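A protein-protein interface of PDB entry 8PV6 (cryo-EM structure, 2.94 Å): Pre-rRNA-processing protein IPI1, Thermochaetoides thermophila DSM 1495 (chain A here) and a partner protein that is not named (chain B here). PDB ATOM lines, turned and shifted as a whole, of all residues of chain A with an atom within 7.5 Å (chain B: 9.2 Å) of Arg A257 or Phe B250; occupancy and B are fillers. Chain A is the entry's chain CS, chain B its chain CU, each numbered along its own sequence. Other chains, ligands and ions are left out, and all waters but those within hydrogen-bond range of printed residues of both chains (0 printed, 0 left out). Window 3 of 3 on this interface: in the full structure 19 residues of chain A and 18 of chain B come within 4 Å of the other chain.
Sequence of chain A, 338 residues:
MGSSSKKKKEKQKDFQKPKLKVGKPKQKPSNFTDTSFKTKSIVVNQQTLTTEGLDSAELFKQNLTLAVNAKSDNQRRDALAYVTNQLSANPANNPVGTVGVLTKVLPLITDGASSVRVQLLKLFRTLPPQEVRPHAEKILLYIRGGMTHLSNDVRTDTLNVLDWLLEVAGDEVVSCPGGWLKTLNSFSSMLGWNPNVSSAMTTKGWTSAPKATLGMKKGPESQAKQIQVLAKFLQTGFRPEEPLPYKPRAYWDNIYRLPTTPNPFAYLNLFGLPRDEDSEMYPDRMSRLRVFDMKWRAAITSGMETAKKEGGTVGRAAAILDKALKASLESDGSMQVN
The guanidinium group of Arg A249 lies within salt-bridge range of the side-chain carboxylate of Asp A253 (2.8 Å).
The side-chain carboxylate (OD2) of Asp A253 lies within salt-bridge range of the guanidinium group (NH1) of Arg A257 (3.5 Å).
The side-chain carboxylate (OD1) of Asp B229 sits at hydrogen-bond distance from the backbone NH (N) of Arg B233.
OD1 of Asp B229 sits at hydrogen-bond distance from N of Ala B234.
The guanidinium group (NE) of Arg B233 is in hydrogen-bond range of the side-chain hydroxyl (OG) of Ser B231 (3.0 Å).
The backbone NH (N) of Met B249 is in hydrogen-bond range of the backbone carbonyl oxygen (O) of Arg B233 (2.9 Å).
Arg A249 touches Glu B252.
O of Asn A254 touches NH2 of Arg B233, at 3.9 Å.
Tyr A256 touches Arg B233.
Tyr A256 touches Phe B250.
Arg A257 touches Phe B250.
OD2 of Asp B229 touches CD2 of Leu A258, at 3.4 Å.
Ala B234 touches Leu A258.
NH1 of Arg B233 touches CD of Pro A259, at 3.8 Å.
The guanidinium group (NH2) of Arg A249 sits at hydrogen-bond distance from the backbone carbonyl oxygen (O) of Gly B251 (3.4 Å).
O of Ile A255 lies within hydrogen-bond range of NE of Arg B233 (2.9 Å).
The backbone carbonyl oxygen (O) of Arg A257 lies within hydrogen-bond range of the guanidinium group (NE) of Arg B233 (3.4 Å).
NE of Arg A257 is in salt-bridge range of OE1 of Glu B248 (3.5 Å).
The side-chain carboxylate (OE2) of Glu B252 is in salt-bridge range of the guanidinium group (NH1) of Arg A257 (2.5 Å).
N of Leu A258 is in hydrogen-bond range of OE2 of Glu B248, at 2.9 Å.
Of chain B, only Arg B233 (3.4 Å), Glu B248 (3.4 Å), Phe B250 (3.4 Å) and Glu B252 (2.5 Å) come within 4 Å of Arg A257.
Of chain A, only Arg A249 comes within 4 Å of Gly B251.
Of the printed residues of chain B, Leu A258 touches Asp B229, Ala B234 and Glu B248.
Printed residues of chain A within 4 Å of Arg B233: Asn A254 (3.9 Å), Ile A255 (2.9 Å), Tyr A256 (3.9 Å), Arg A257 (3.4 Å) and Pro A259 (3.8 Å).
Of the printed residues of chain B, Asn A254 touches Arg B233.
Printed residues of chain A within 4 Å of Asp B229: Leu A258 (3.4 Å).
The nearest printed residue of chain B that does not touch Leu A258 is Arg B233 (4.1 Å).
Of the 24 printed residues of chain B, 7 touch a printed residue of chain A.
Hydrophobic or aromatic side chains of chain A that line the printed part of chain B: Tyr A256, Leu A258 and Pro A259.
Among the printed residues, 14 pairs touch across the chains.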
ATOM      1  N   ARG A 249     -33.545 -15.722   2.296  1.00  0.00           N
ATOM      2  CA  ARG A 249     -32.240 -15.144   2.586  1.00  0.00           C
ATOM      3  C   ARG A 249     -32.402 -13.799   3.296  1.00  0.00           C
ATOM      4  O   ARG A 249     -31.771 -12.800   2.970  1.00  0.00           O
ATOM      5  CB  ARG A 249     -31.409 -15.011   1.311  1.00  0.00           C
ATOM      6  CG  ARG A 249     -32.092 -14.282   0.164  1.00  0.00           C
ATOM      7  CD  ARG A 249     -31.083 -13.965  -0.919  1.00  0.00           C
ATOM      8  NE  ARG A 249     -30.048 -13.069  -0.420  1.00  0.00           N
ATOM      9  CZ  ARG A 249     -28.852 -12.923  -0.972  1.00  0.00           C
ATOM     10  NH1 ARG A 249     -28.503 -13.597  -2.055  1.00  0.00           N
ATOM     11  NH2 ARG A 249     -27.982 -12.081  -0.421  1.00  0.00           N
ATOM     12  N   TRP A 252     -29.781 -14.120   7.302  1.00  0.00           N
ATOM     13  CA  TRP A 252     -28.347 -13.918   7.145  1.00  0.00           C
ATOM     14  C   TRP A 252     -28.005 -12.585   6.495  1.00  0.00           C
ATOM     15  O   TRP A 252     -26.962 -12.006   6.822  1.00  0.00           O
ATOM     16  CB  TRP A 252     -27.734 -15.069   6.345  1.00  0.00           C
ATOM     17  CG  TRP A 252     -27.487 -16.282   7.189  1.00  0.00           C
ATOM     18  CD1 TRP A 252     -28.071 -17.505   7.052  1.00  0.00           C
ATOM     19  CD2 TRP A 252     -26.602 -16.383   8.314  1.00  0.00           C
ATOM     20  NE1 TRP A 252     -27.603 -18.364   8.017  1.00  0.00           N
ATOM     21  CE2 TRP A 252     -26.700 -17.698   8.803  1.00  0.00           C
ATOM     22  CE3 TRP A 252     -25.734 -15.491   8.951  1.00  0.00           C
ATOM     23  CZ2 TRP A 252     -25.966 -18.141   9.899  1.00  0.00           C
ATOM     24  CZ3 TRP A 252     -25.008 -15.934  10.038  1.00  0.00           C
ATOM     25  CH2 TRP A 252     -25.127 -17.247  10.501  1.00  0.00           C
ATOM     26  N   ASP A 253     -28.845 -12.088   5.587  1.00  0.00           N
ATOM     27  CA  ASP A 253     -28.638 -10.763   5.021  1.00  0.00           C
ATOM     28  C   ASP A 253     -28.837  -9.652   6.037  1.00  0.00           C
ATOM     29  O   ASP A 253     -28.186  -8.608   5.922  1.00  0.00           O
ATOM     30  CB  ASP A 253     -29.568 -10.534   3.828  1.00  0.00           C
ATOM     31  CG  ASP A 253     -29.120 -11.289   2.594  1.00  0.00           C
ATOM     32  OD1 ASP A 253     -28.215 -12.140   2.713  1.00  0.00           O
ATOM     33  OD2 ASP A 253     -29.673 -11.032   1.505  1.00  0.00           O
ATOM     34  N   ASN A 254     -29.689  -9.863   7.041  1.00  0.00           N
ATOM     35  CA  ASN A 254     -29.832  -8.928   8.148  1.00  0.00           C
ATOM     36  C   ASN A 254     -28.549  -8.761   8.953  1.00  0.00           C
ATOM     37  O   ASN A 254     -28.377  -7.728   9.607  1.00  0.00           O
ATOM     38  CB  ASN A 254     -30.963  -9.391   9.071  1.00  0.00           C
ATOM     39  CG  ASN A 254     -31.402  -8.317  10.044  1.00  0.00           C
ATOM     40  OD1 ASN A 254     -31.515  -7.146   9.685  1.00  0.00           O
ATOM     41  ND2 ASN A 254     -31.652  -8.711  11.284  1.00  0.00           N
ATOM     42  N   ILE A 255     -27.643  -9.736   8.909  1.00  0.00           N
ATOM     43  CA  ILE A 255     -26.395  -9.669   9.656  1.00  0.00           C
ATOM     44  C   ILE A 255     -25.266  -9.232   8.733  1.00  0.00           C
ATOM     45  O   ILE A 255     -24.403  -8.437   9.123  1.00  0.00           O
ATOM     46  CB  ILE A 255     -26.074 -11.022  10.317  1.00  0.00           C
ATOM     47  CG1 ILE A 255     -27.293 -11.546  11.075  1.00  0.00           C
ATOM     48  CG2 ILE A 255     -24.896 -10.891  11.260  1.00  0.00           C
ATOM     49  CD1 ILE A 255     -27.073 -12.892  11.729  1.00  0.00           C
ATOM     50  N   TYR A 256     -25.264  -9.735   7.501  1.00  0.00           N
ATOM     51  CA  TYR A 256     -24.145  -9.520   6.594  1.00  0.00           C
ATOM     52  C   TYR A 256     -24.386  -8.438   5.550  1.00  0.00           C
ATOM     53  O   TYR A 256     -23.589  -8.324   4.614  1.00  0.00           O
ATOM     54  CB  TYR A 256     -23.781 -10.830   5.891  1.00  0.00           C
ATOM     55  CG  TYR A 256     -23.083 -11.816   6.794  1.00  0.00           C
ATOM     56  CD1 TYR A 256     -22.146 -11.388   7.723  1.00  0.00           C
ATOM     57  CD2 TYR A 256     -23.362 -13.172   6.721  1.00  0.00           C
ATOM     58  CE1 TYR A 256     -21.505 -12.282   8.554  1.00  0.00           C
ATOM     59  CE2 TYR A 256     -22.726 -14.075   7.548  1.00  0.00           C
ATOM     60  CZ  TYR A 256     -21.800 -13.623   8.462  1.00  0.00           C
ATOM     61  OH  TYR A 256     -21.162 -14.519   9.288  1.00  0.00           O
ATOM     62  N   ARG A 257     -25.450  -7.645   5.669  1.00  0.00           N
ATOM     63  CA  ARG A 257     -25.681  -6.534   4.759  1.00  0.00           C
ATOM     64  C   ARG A 257     -26.062  -5.291   5.546  1.00  0.00           C
ATOM     65  O   ARG A 257     -26.404  -5.368   6.729  1.00  0.00           O
ATOM     66  CB  ARG A 257     -26.768  -6.857   3.729  1.00  0.00           C
ATOM     67  CG  ARG A 257     -26.389  -7.957   2.755  1.00  0.00           C
ATOM     68  CD  ARG A 257     -27.496  -8.231   1.759  1.00  0.00           C
ATOM     69  NE  ARG A 257     -27.728  -7.090   0.885  1.00  0.00           N
ATOM     70  CZ  ARG A 257     -28.629  -7.064  -0.088  1.00  0.00           C
ATOM     71  NH1 ARG A 257     -29.398  -8.108  -0.344  1.00  0.00           N
ATOM     72  NH2 ARG A 257     -28.756  -5.964  -0.824  1.00  0.00           N
ATOM     73  N   LEU A 258     -25.983  -4.142   4.879  1.00  0.00           N
ATOM     74  CA  LEU A 258     -26.305  -2.877   5.515  1.00  0.00           C
ATOM     75  C   LEU A 258     -27.802  -2.795   5.816  1.00  0.00           C
ATOM     76  O   LEU A 258     -28.615  -3.412   5.123  1.00  0.00           O
ATOM     77  CB  LEU A 258     -25.893  -1.711   4.623  1.00  0.00           C
ATOM     78  CG  LEU A 258     -24.398  -1.453   4.447  1.00  0.00           C
ATOM     79  CD1 LEU A 258     -24.189  -0.328   3.455  1.00  0.00           C
ATOM     80  CD2 LEU A 258     -23.749  -1.121   5.775  1.00  0.00           C
ATOM     81  N   PRO A 259     -28.187  -2.056   6.856  1.00  0.00           N
ATOM     82  CA  PRO A 259     -29.616  -1.902   7.158  1.00  0.00           C
ATOM     83  C   PRO A 259     -30.325  -1.086   6.087  1.00  0.00           C
ATOM     84  O   PRO A 259     -29.954   0.054   5.801  1.00  0.00           O
ATOM     85  CB  PRO A 259     -29.615  -1.178   8.510  1.00  0.00           C
ATOM     86  CG  PRO A 259     -28.278  -1.478   9.097  1.00  0.00           C
ATOM     87  CD  PRO A 259     -27.344  -1.509   7.931  1.00  0.00           C
ATOM     88  N   THR A 260     -31.354  -1.685   5.493  1.00  0.00           N
ATOM     89  CA  THR A 260     -32.135  -1.044   4.446  1.00  0.00           C
ATOM     90  C   THR A 260     -33.327  -0.267   4.986  1.00  0.00           C
ATOM     91  O   THR A 260     -33.970   0.463   4.225  1.00  0.00           O
ATOM     92  CB  THR A 260     -32.623  -2.088   3.438  1.00  0.00           C
ATOM     93  OG1 THR A 260     -33.556  -2.969   4.074  1.00  0.00           O
ATOM     94  CG2 THR A 260     -31.452  -2.900   2.909  1.00  0.00           C
ATOM     95  N   SER B 184      -9.500  -4.170   7.243  1.00  0.00           N
ATOM     96  CA  SER B 184     -10.510  -4.718   8.129  1.00  0.00           C
ATOM     97  C   SER B 184      -9.982  -4.741   9.563  1.00  0.00           C
ATOM     98  O   SER B 184      -8.772  -4.852   9.784  1.00  0.00           O
ATOM     99  CB  SER B 184     -10.896  -6.126   7.681  1.00  0.00           C
ATOM    100  OG  SER B 184     -11.558  -6.838   8.710  1.00  0.00           O
ATOM    101  N   THR B 191      -9.219 -14.357   7.581  1.00  0.00           N
ATOM    102  CA  THR B 191     -10.420 -13.535   7.550  1.00  0.00           C
ATOM    103  C   THR B 191     -10.157 -12.053   7.330  1.00  0.00           C
ATOM    104  O   THR B 191     -11.099 -11.322   7.010  1.00  0.00           O
ATOM    105  CB  THR B 191     -11.215 -13.698   8.853  1.00  0.00           C
ATOM    106  OG1 THR B 191     -10.459 -13.163   9.945  1.00  0.00           O
ATOM    107  CG2 THR B 191     -11.507 -15.162   9.117  1.00  0.00           C
ATOM    108  N   PHE B 193      -8.687  -8.541   5.517  1.00  0.00           N
ATOM    109  CA  PHE B 193      -8.505  -8.047   4.163  1.00  0.00           C
ATOM    110  C   PHE B 193      -8.155  -6.567   4.200  1.00  0.00           C
ATOM    111  O   PHE B 193      -8.301  -5.898   5.226  1.00  0.00           O
ATOM    112  CB  PHE B 193      -9.752  -8.291   3.287  1.00  0.00           C
ATOM    113  CG  PHE B 193     -11.006  -7.620   3.783  1.00  0.00           C
ATOM    114  CD1 PHE B 193     -11.337  -6.336   3.378  1.00  0.00           C
ATOM    115  CD2 PHE B 193     -11.864  -8.286   4.639  1.00  0.00           C
ATOM    116  CE1 PHE B 193     -12.487  -5.730   3.830  1.00  0.00           C
ATOM    117  CE2 PHE B 193     -13.017  -7.683   5.092  1.00  0.00           C
ATOM    118  CZ  PHE B 193     -13.327  -6.404   4.685  1.00  0.00           C
ATOM    119  N   ILE B 205      -9.089  -5.811  -3.231  1.00  0.00           N
ATOM    120  CA  ILE B 205      -9.162  -6.403  -1.902  1.00  0.00           C
ATOM    121  C   ILE B 205      -8.149  -7.534  -1.833  1.00  0.00           C
ATOM    122  O   ILE B 205      -8.233  -8.504  -2.601  1.00  0.00           O
ATOM    123  CB  ILE B 205     -10.578  -6.914  -1.593  1.00  0.00           C
ATOM    124  CG1 ILE B 205     -11.629  -5.902  -2.043  1.00  0.00           C
ATOM    125  CG2 ILE B 205     -10.728  -7.204  -0.117  1.00  0.00           C
ATOM    126  CD1 ILE B 205     -13.047  -6.386  -1.858  1.00  0.00           C
ATOM    127  N   ASP B 229     -17.495   0.315   6.204  1.00  0.00           N
ATOM    128  CA  ASP B 229     -18.504   0.449   7.233  1.00  0.00           C
ATOM    129  C   ASP B 229     -18.017  -0.280   8.484  1.00  0.00           C
ATOM    130  O   ASP B 229     -17.194  -1.192   8.390  1.00  0.00           O
ATOM    131  CB  ASP B 229     -19.844  -0.102   6.750  1.00  0.00           C
ATOM    132  CG  ASP B 229     -19.865  -1.600   6.688  1.00  0.00           C
ATOM    133  OD1 ASP B 229     -18.924  -2.181   6.113  1.00  0.00           O
ATOM    134  OD2 ASP B 229     -20.821  -2.204   7.217  1.00  0.00           O
ATOM    135  N   SER B 231     -19.251  -2.493  10.424  1.00  0.00           N
ATOM    136  CA  SER B 231     -19.521  -3.922  10.534  1.00  0.00           C
ATOM    137  C   SER B 231     -18.892  -4.699   9.384  1.00  0.00           C
ATOM    138  O   SER B 231     -19.206  -5.879   9.185  1.00  0.00           O
ATOM    139  CB  SER B 231     -21.026  -4.165  10.589  1.00  0.00           C
ATOM    140  OG  SER B 231     -21.317  -5.549  10.541  1.00  0.00           O
ATOM    141  N   SER B 232     -18.024  -4.041   8.605  1.00  0.00           N
ATOM    142  CA  SER B 232     -17.248  -4.632   7.515  1.00  0.00           C
ATOM    143  C   SER B 232     -18.130  -5.223   6.419  1.00  0.00           C
ATOM    144  O   SER B 232     -17.745  -6.198   5.765  1.00  0.00           O
ATOM    145  CB  SER B 232     -16.282  -5.692   8.054  1.00  0.00           C
ATOM    146  OG  SER B 232     -15.415  -6.153   7.037  1.00  0.00           O
ATOM    147  N   ARG B 233     -19.312  -4.639   6.206  1.00  0.00           N
ATOM    148  CA  ARG B 233     -20.228  -5.163   5.197  1.00  0.00           C
ATOM    149  C   ARG B 233     -20.056  -4.456   3.858  1.00  0.00           C
ATOM    150  O   ARG B 233     -20.406  -5.012   2.811  1.00  0.00           O
ATOM    151  CB  ARG B 233     -21.674  -5.022   5.667  1.00  0.00           C
ATOM    152  CG  ARG B 233     -21.983  -5.652   7.002  1.00  0.00           C
ATOM    153  CD  ARG B 233     -23.099  -4.889   7.687  1.00  0.00           C
ATOM    154  NE  ARG B 233     -23.723  -5.657   8.755  1.00  0.00           N
ATOM    155  CZ  ARG B 233     -24.545  -5.146   9.660  1.00  0.00           C
ATOM    156  NH1 ARG B 233     -24.851  -3.861   9.667  1.00  0.00           N
ATOM    157  NH2 ARG B 233     -25.071  -5.945  10.583  1.00  0.00           N
ATOM    158  N   ALA B 234     -19.552  -3.223   3.866  1.00  0.00           N
ATOM    159  CA  ALA B 234     -19.545  -2.423   2.652  1.00  0.00           C
ATOM    160  C   ALA B 234     -18.372  -1.453   2.640  1.00  0.00           C
ATOM    161  O   ALA B 234     -17.787  -1.124   3.675  1.00  0.00           O
ATOM    162  CB  ALA B 234     -20.854  -1.646   2.486  1.00  0.00           C
ATOM    163  N   ILE B 235     -18.058  -0.990   1.433  1.00  0.00           N
ATOM    164  CA  ILE B 235     -16.985  -0.043   1.168  1.00  0.00           C
ATOM    165  C   ILE B 235     -17.622   1.203   0.568  1.00  0.00           C
ATOM    166  O   ILE B 235     -18.358   1.105  -0.420  1.00  0.00           O
ATOM    167  CB  ILE B 235     -15.951  -0.624   0.188  1.00  0.00           C
ATOM    168  CG1 ILE B 235     -15.386  -1.944   0.701  1.00  0.00           C
ATOM    169  CG2 ILE B 235     -14.809   0.347  -0.004  1.00  0.00           C
ATOM    170  CD1 ILE B 235     -14.671  -1.831   1.991  1.00  0.00           C
ATOM    171  N   ALA B 247     -20.070  -0.345  -2.256  1.00  0.00           N
ATOM    172  CA  ALA B 247     -19.855  -1.704  -2.730  1.00  0.00           C
ATOM    173  C   ALA B 247     -20.067  -2.660  -1.569  1.00  0.00           C
ATOM    174  O   ALA B 247     -19.349  -2.590  -0.568  1.00  0.00           O
ATOM    175  CB  ALA B 247     -18.451  -1.872  -3.310  1.00  0.00           C
ATOM    176  N   GLU B 248     -21.042  -3.550  -1.704  1.00  0.00           N
ATOM    177  CA  GLU B 248     -21.446  -4.436  -0.622  1.00  0.00           C
ATOM    178  C   GLU B 248     -20.785  -5.792  -0.826  1.00  0.00           C
ATOM    179  O   GLU B 248     -20.875  -6.373  -1.913  1.00  0.00           O
ATOM    180  CB  GLU B 248     -22.967  -4.563  -0.566  1.00  0.00           C
ATOM    181  CG  GLU B 248     -23.511  -4.797   0.831  1.00  0.00           C
ATOM    182  CD  GLU B 248     -24.982  -4.454   0.945  1.00  0.00           C
ATOM    183  OE1 GLU B 248     -25.670  -4.420  -0.097  1.00  0.00           O
ATOM    184  OE2 GLU B 248     -25.450  -4.218   2.078  1.00  0.00           O
ATOM    185  N   MET B 249     -20.112  -6.284   0.220  1.00  0.00           N
ATOM    186  CA  MET B 249     -19.352  -7.525   0.114  1.00  0.00           C
ATOM    187  C   MET B 249     -20.265  -8.730  -0.077  1.00  0.00           C
ATOM    188  O   MET B 249     -19.933  -9.655  -0.827  1.00  0.00           O
ATOM    189  CB  MET B 249     -18.492  -7.713   1.363  1.00  0.00           C
ATOM    190  CG  MET B 249     -17.389  -6.683   1.573  1.00  0.00           C
ATOM    191  SD  MET B 249     -16.136  -6.623   0.278  1.00  0.00           S
ATOM    192  CE  MET B 249     -16.637  -5.168  -0.638  1.00  0.00           C
ATOM    193  N   PHE B 250     -21.415  -8.740   0.594  1.00  0.00           N
ATOM    194  CA  PHE B 250     -22.248  -9.930   0.699  1.00  0.00           C
ATOM    195  C   PHE B 250     -23.652  -9.725   0.145  1.00  0.00           C
ATOM    196  O   PHE B 250     -24.630 -10.116   0.791  1.00  0.00           O
ATOM    197  CB  PHE B 250     -22.310 -10.383   2.156  1.00  0.00           C
ATOM    198  CG  PHE B 250     -20.970 -10.417   2.831  1.00  0.00           C
ATOM    199  CD1 PHE B 250     -19.982 -11.282   2.396  1.00  0.00           C
ATOM    200  CD2 PHE B 250     -20.693  -9.571   3.891  1.00  0.00           C
ATOM    201  CE1 PHE B 250     -18.746 -11.311   3.013  1.00  0.00           C
ATOM    202  CE2 PHE B 250     -19.458  -9.595   4.511  1.00  0.00           C
ATOM    203  CZ  PHE B 250     -18.485 -10.465   4.071  1.00  0.00           C
ATOM    204  N   GLY B 251     -23.776  -9.128  -1.035  1.00  0.00           N
ATOM    205  CA  GLY B 251     -25.076  -8.937  -1.642  1.00  0.00           C
ATOM    206  C   GLY B 251     -25.568 -10.179  -2.361  1.00  0.00           C
ATOM    207  O   GLY B 251     -25.141 -11.305  -2.102  1.00  0.00           O
ATOM    208  N   GLU B 252     -26.515  -9.958  -3.277  1.00  0.00           N
ATOM    209  CA  GLU B 252     -27.014 -11.050  -4.110  1.00  0.00           C
ATOM    210  C   GLU B 252     -25.925 -11.577  -5.033  1.00  0.00           C
ATOM    211  O   GLU B 252     -25.832 -12.788  -5.270  1.00  0.00           O
ATOM    212  CB  GLU B 252     -28.230 -10.591  -4.915  1.00  0.00           C
ATOM    213  CG  GLU B 252     -29.468 -10.301  -4.077  1.00  0.00           C
ATOM    214  CD  GLU B 252     -29.477  -8.899  -3.501  1.00  0.00           C
ATOM    215  OE1 GLU B 252     -28.645  -8.073  -3.932  1.00  0.00           O
ATOM    216  OE2 GLU B 252     -30.311  -8.625  -2.613  1.00  0.00           O
ATOM    217  N   LYS B 253     -25.101 -10.682  -5.576  1.00  0.00           N
ATOM    218  CA  LYS B 253     -23.875 -11.074  -6.250  1.00  0.00           C
ATOM    219  C   LYS B 253     -22.706 -10.707  -5.354  1.00  0.00           C
ATOM    220  O   LYS B 253     -22.195  -9.580  -5.451  1.00  0.00           O
ATOM    221  CB  LYS B 253     -23.752 -10.378  -7.600  1.00  0.00           C
ATOM    222  CG  LYS B 253     -22.557 -10.822  -8.429  1.00  0.00           C
ATOM    223  CD  LYS B 253     -22.675 -12.285  -8.820  1.00  0.00           C
ATOM    224  CE  LYS B 253     -23.797 -12.494  -9.823  1.00  0.00           C
ATOM    225  NZ  LYS B 253     -23.893 -13.913 -10.264  1.00  0.00           N
ATOM    226  N   PRO B 254     -22.267 -11.594  -4.461  1.00  0.00           N
ATOM    227  CA  PRO B 254     -21.298 -11.190  -3.434  1.00  0.00           C
ATOM    228  C   PRO B 254     -19.885 -11.027  -3.963  1.00  0.00           C
ATOM    229  O   PRO B 254     -19.416 -11.821  -4.784  1.00  0.00           O
ATOM    230  CB  PRO B 254     -21.382 -12.327  -2.412  1.00  0.00           C
ATOM    231  CG  PRO B 254     -21.798 -13.505  -3.207  1.00  0.00           C
ATOM    232  CD  PRO B 254     -22.701 -12.992  -4.293  1.00  0.00           C
ATOM    233  N   LEU B 255     -19.199  -9.982  -3.497  1.00  0.00           N
ATOM    234  CA  LEU B 255     -17.805  -9.786  -3.874  1.00  0.00           C
ATOM    235  C   LEU B 255     -16.895 -10.734  -3.104  1.00  0.00           C
ATOM    236  O   LEU B 255     -15.856 -11.165  -3.618  1.00  0.00           O
ATOM    237  CB  LEU B 255     -17.404  -8.332  -3.642  1.00  0.00           C
ATOM    238  CG  LEU B 255     -18.322  -7.304  -4.305  1.00  0.00           C
ATOM    239  CD1 LEU B 255     -17.827  -5.895  -4.064  1.00  0.00           C
ATOM    240  CD2 LEU B 255     -18.447  -7.575  -5.795  1.00  0.00           C
ATOM    241  N   LEU B 256     -17.268 -11.067  -1.873  1.00  0.00           N
ATOM    242  CA  LEU B 256     -16.538 -12.022  -1.055  1.00  0.00           C
ATOM    243  C   LEU B 256     -17.514 -13.028  -0.468  1.00  0.00           C
ATOM    244  O   LEU B 256     -18.719 -12.782  -0.386  1.00  0.00           O
ATOM    245  CB  LEU B 256     -15.760 -11.329   0.072  1.00  0.00           C
ATOM    246  CG  LEU B 256     -14.561 -10.471  -0.331  1.00  0.00           C
ATOM    247  CD1 LEU B 256     -13.885  -9.912   0.902  1.00  0.00           C
ATOM    248  CD2 LEU B 256     -13.582 -11.284  -1.152  1.00  0.00           C
ATOM    249  N   GLY B 257     -16.978 -14.172  -0.053  1.00  0.00           N
ATOM    250  CA  GLY B 257     -17.784 -15.207   0.545  1.00  0.00           C
ATOM    251  C   GLY B 257     -17.892 -16.444  -0.322  1.00  0.00           C
ATOM    252  O   GLY B 257     -17.292 -16.532  -1.398  1.00  0.00           O
ATOM    253  N   PRO B 258     -18.648 -17.440   0.153  1.00  0.00           N
ATOM    254  CA  PRO B 258     -18.784 -18.691  -0.615  1.00  0.00           C
ATOM    255  C   PRO B 258     -19.500 -18.525  -1.946  1.00  0.00           C
ATOM    256  O   PRO B 258     -19.179 -19.234  -2.907  1.00  0.00           O
ATOM    257  CB  PRO B 258     -19.571 -19.595   0.342  1.00  0.00           C
ATOM    258  CG  PRO B 258     -20.301 -18.651   1.237  1.00  0.00           C
ATOM    259  CD  PRO B 258     -19.375 -17.495   1.432  1.00  0.00           C
ATOM    260  N   GLY B 259     -20.462 -17.607  -2.031  1.00  0.00           N
ATOM    261  CA  GLY B 259     -21.209 -17.451  -3.268  1.00  0.00           C
ATOM    262  C   GLY B 259     -20.491 -16.589  -4.288  1.00  0.00           C
ATOM    263  O   GLY B 259     -20.976 -16.398  -5.405  1.00  0.00           O
ATOM    264  N   SER B 260     -19.332 -16.051  -3.916  1.00  0.00           N
ATOM    265  CA  SER B 260     -18.597 -15.155  -4.797  1.00  0.00           C
ATOM    266  C   SER B 260     -17.992 -15.921  -5.968  1.00  0.00           C
ATOM    267  O   SER B 260     -17.777 -17.133  -5.906  1.00  0.00           O
ATOM    268  CB  SER B 260     -17.497 -14.432  -4.022  1.00  0.00           C
ATOM    269  OG  SER B 260     -16.427 -15.310  -3.724  1.00  0.00           O
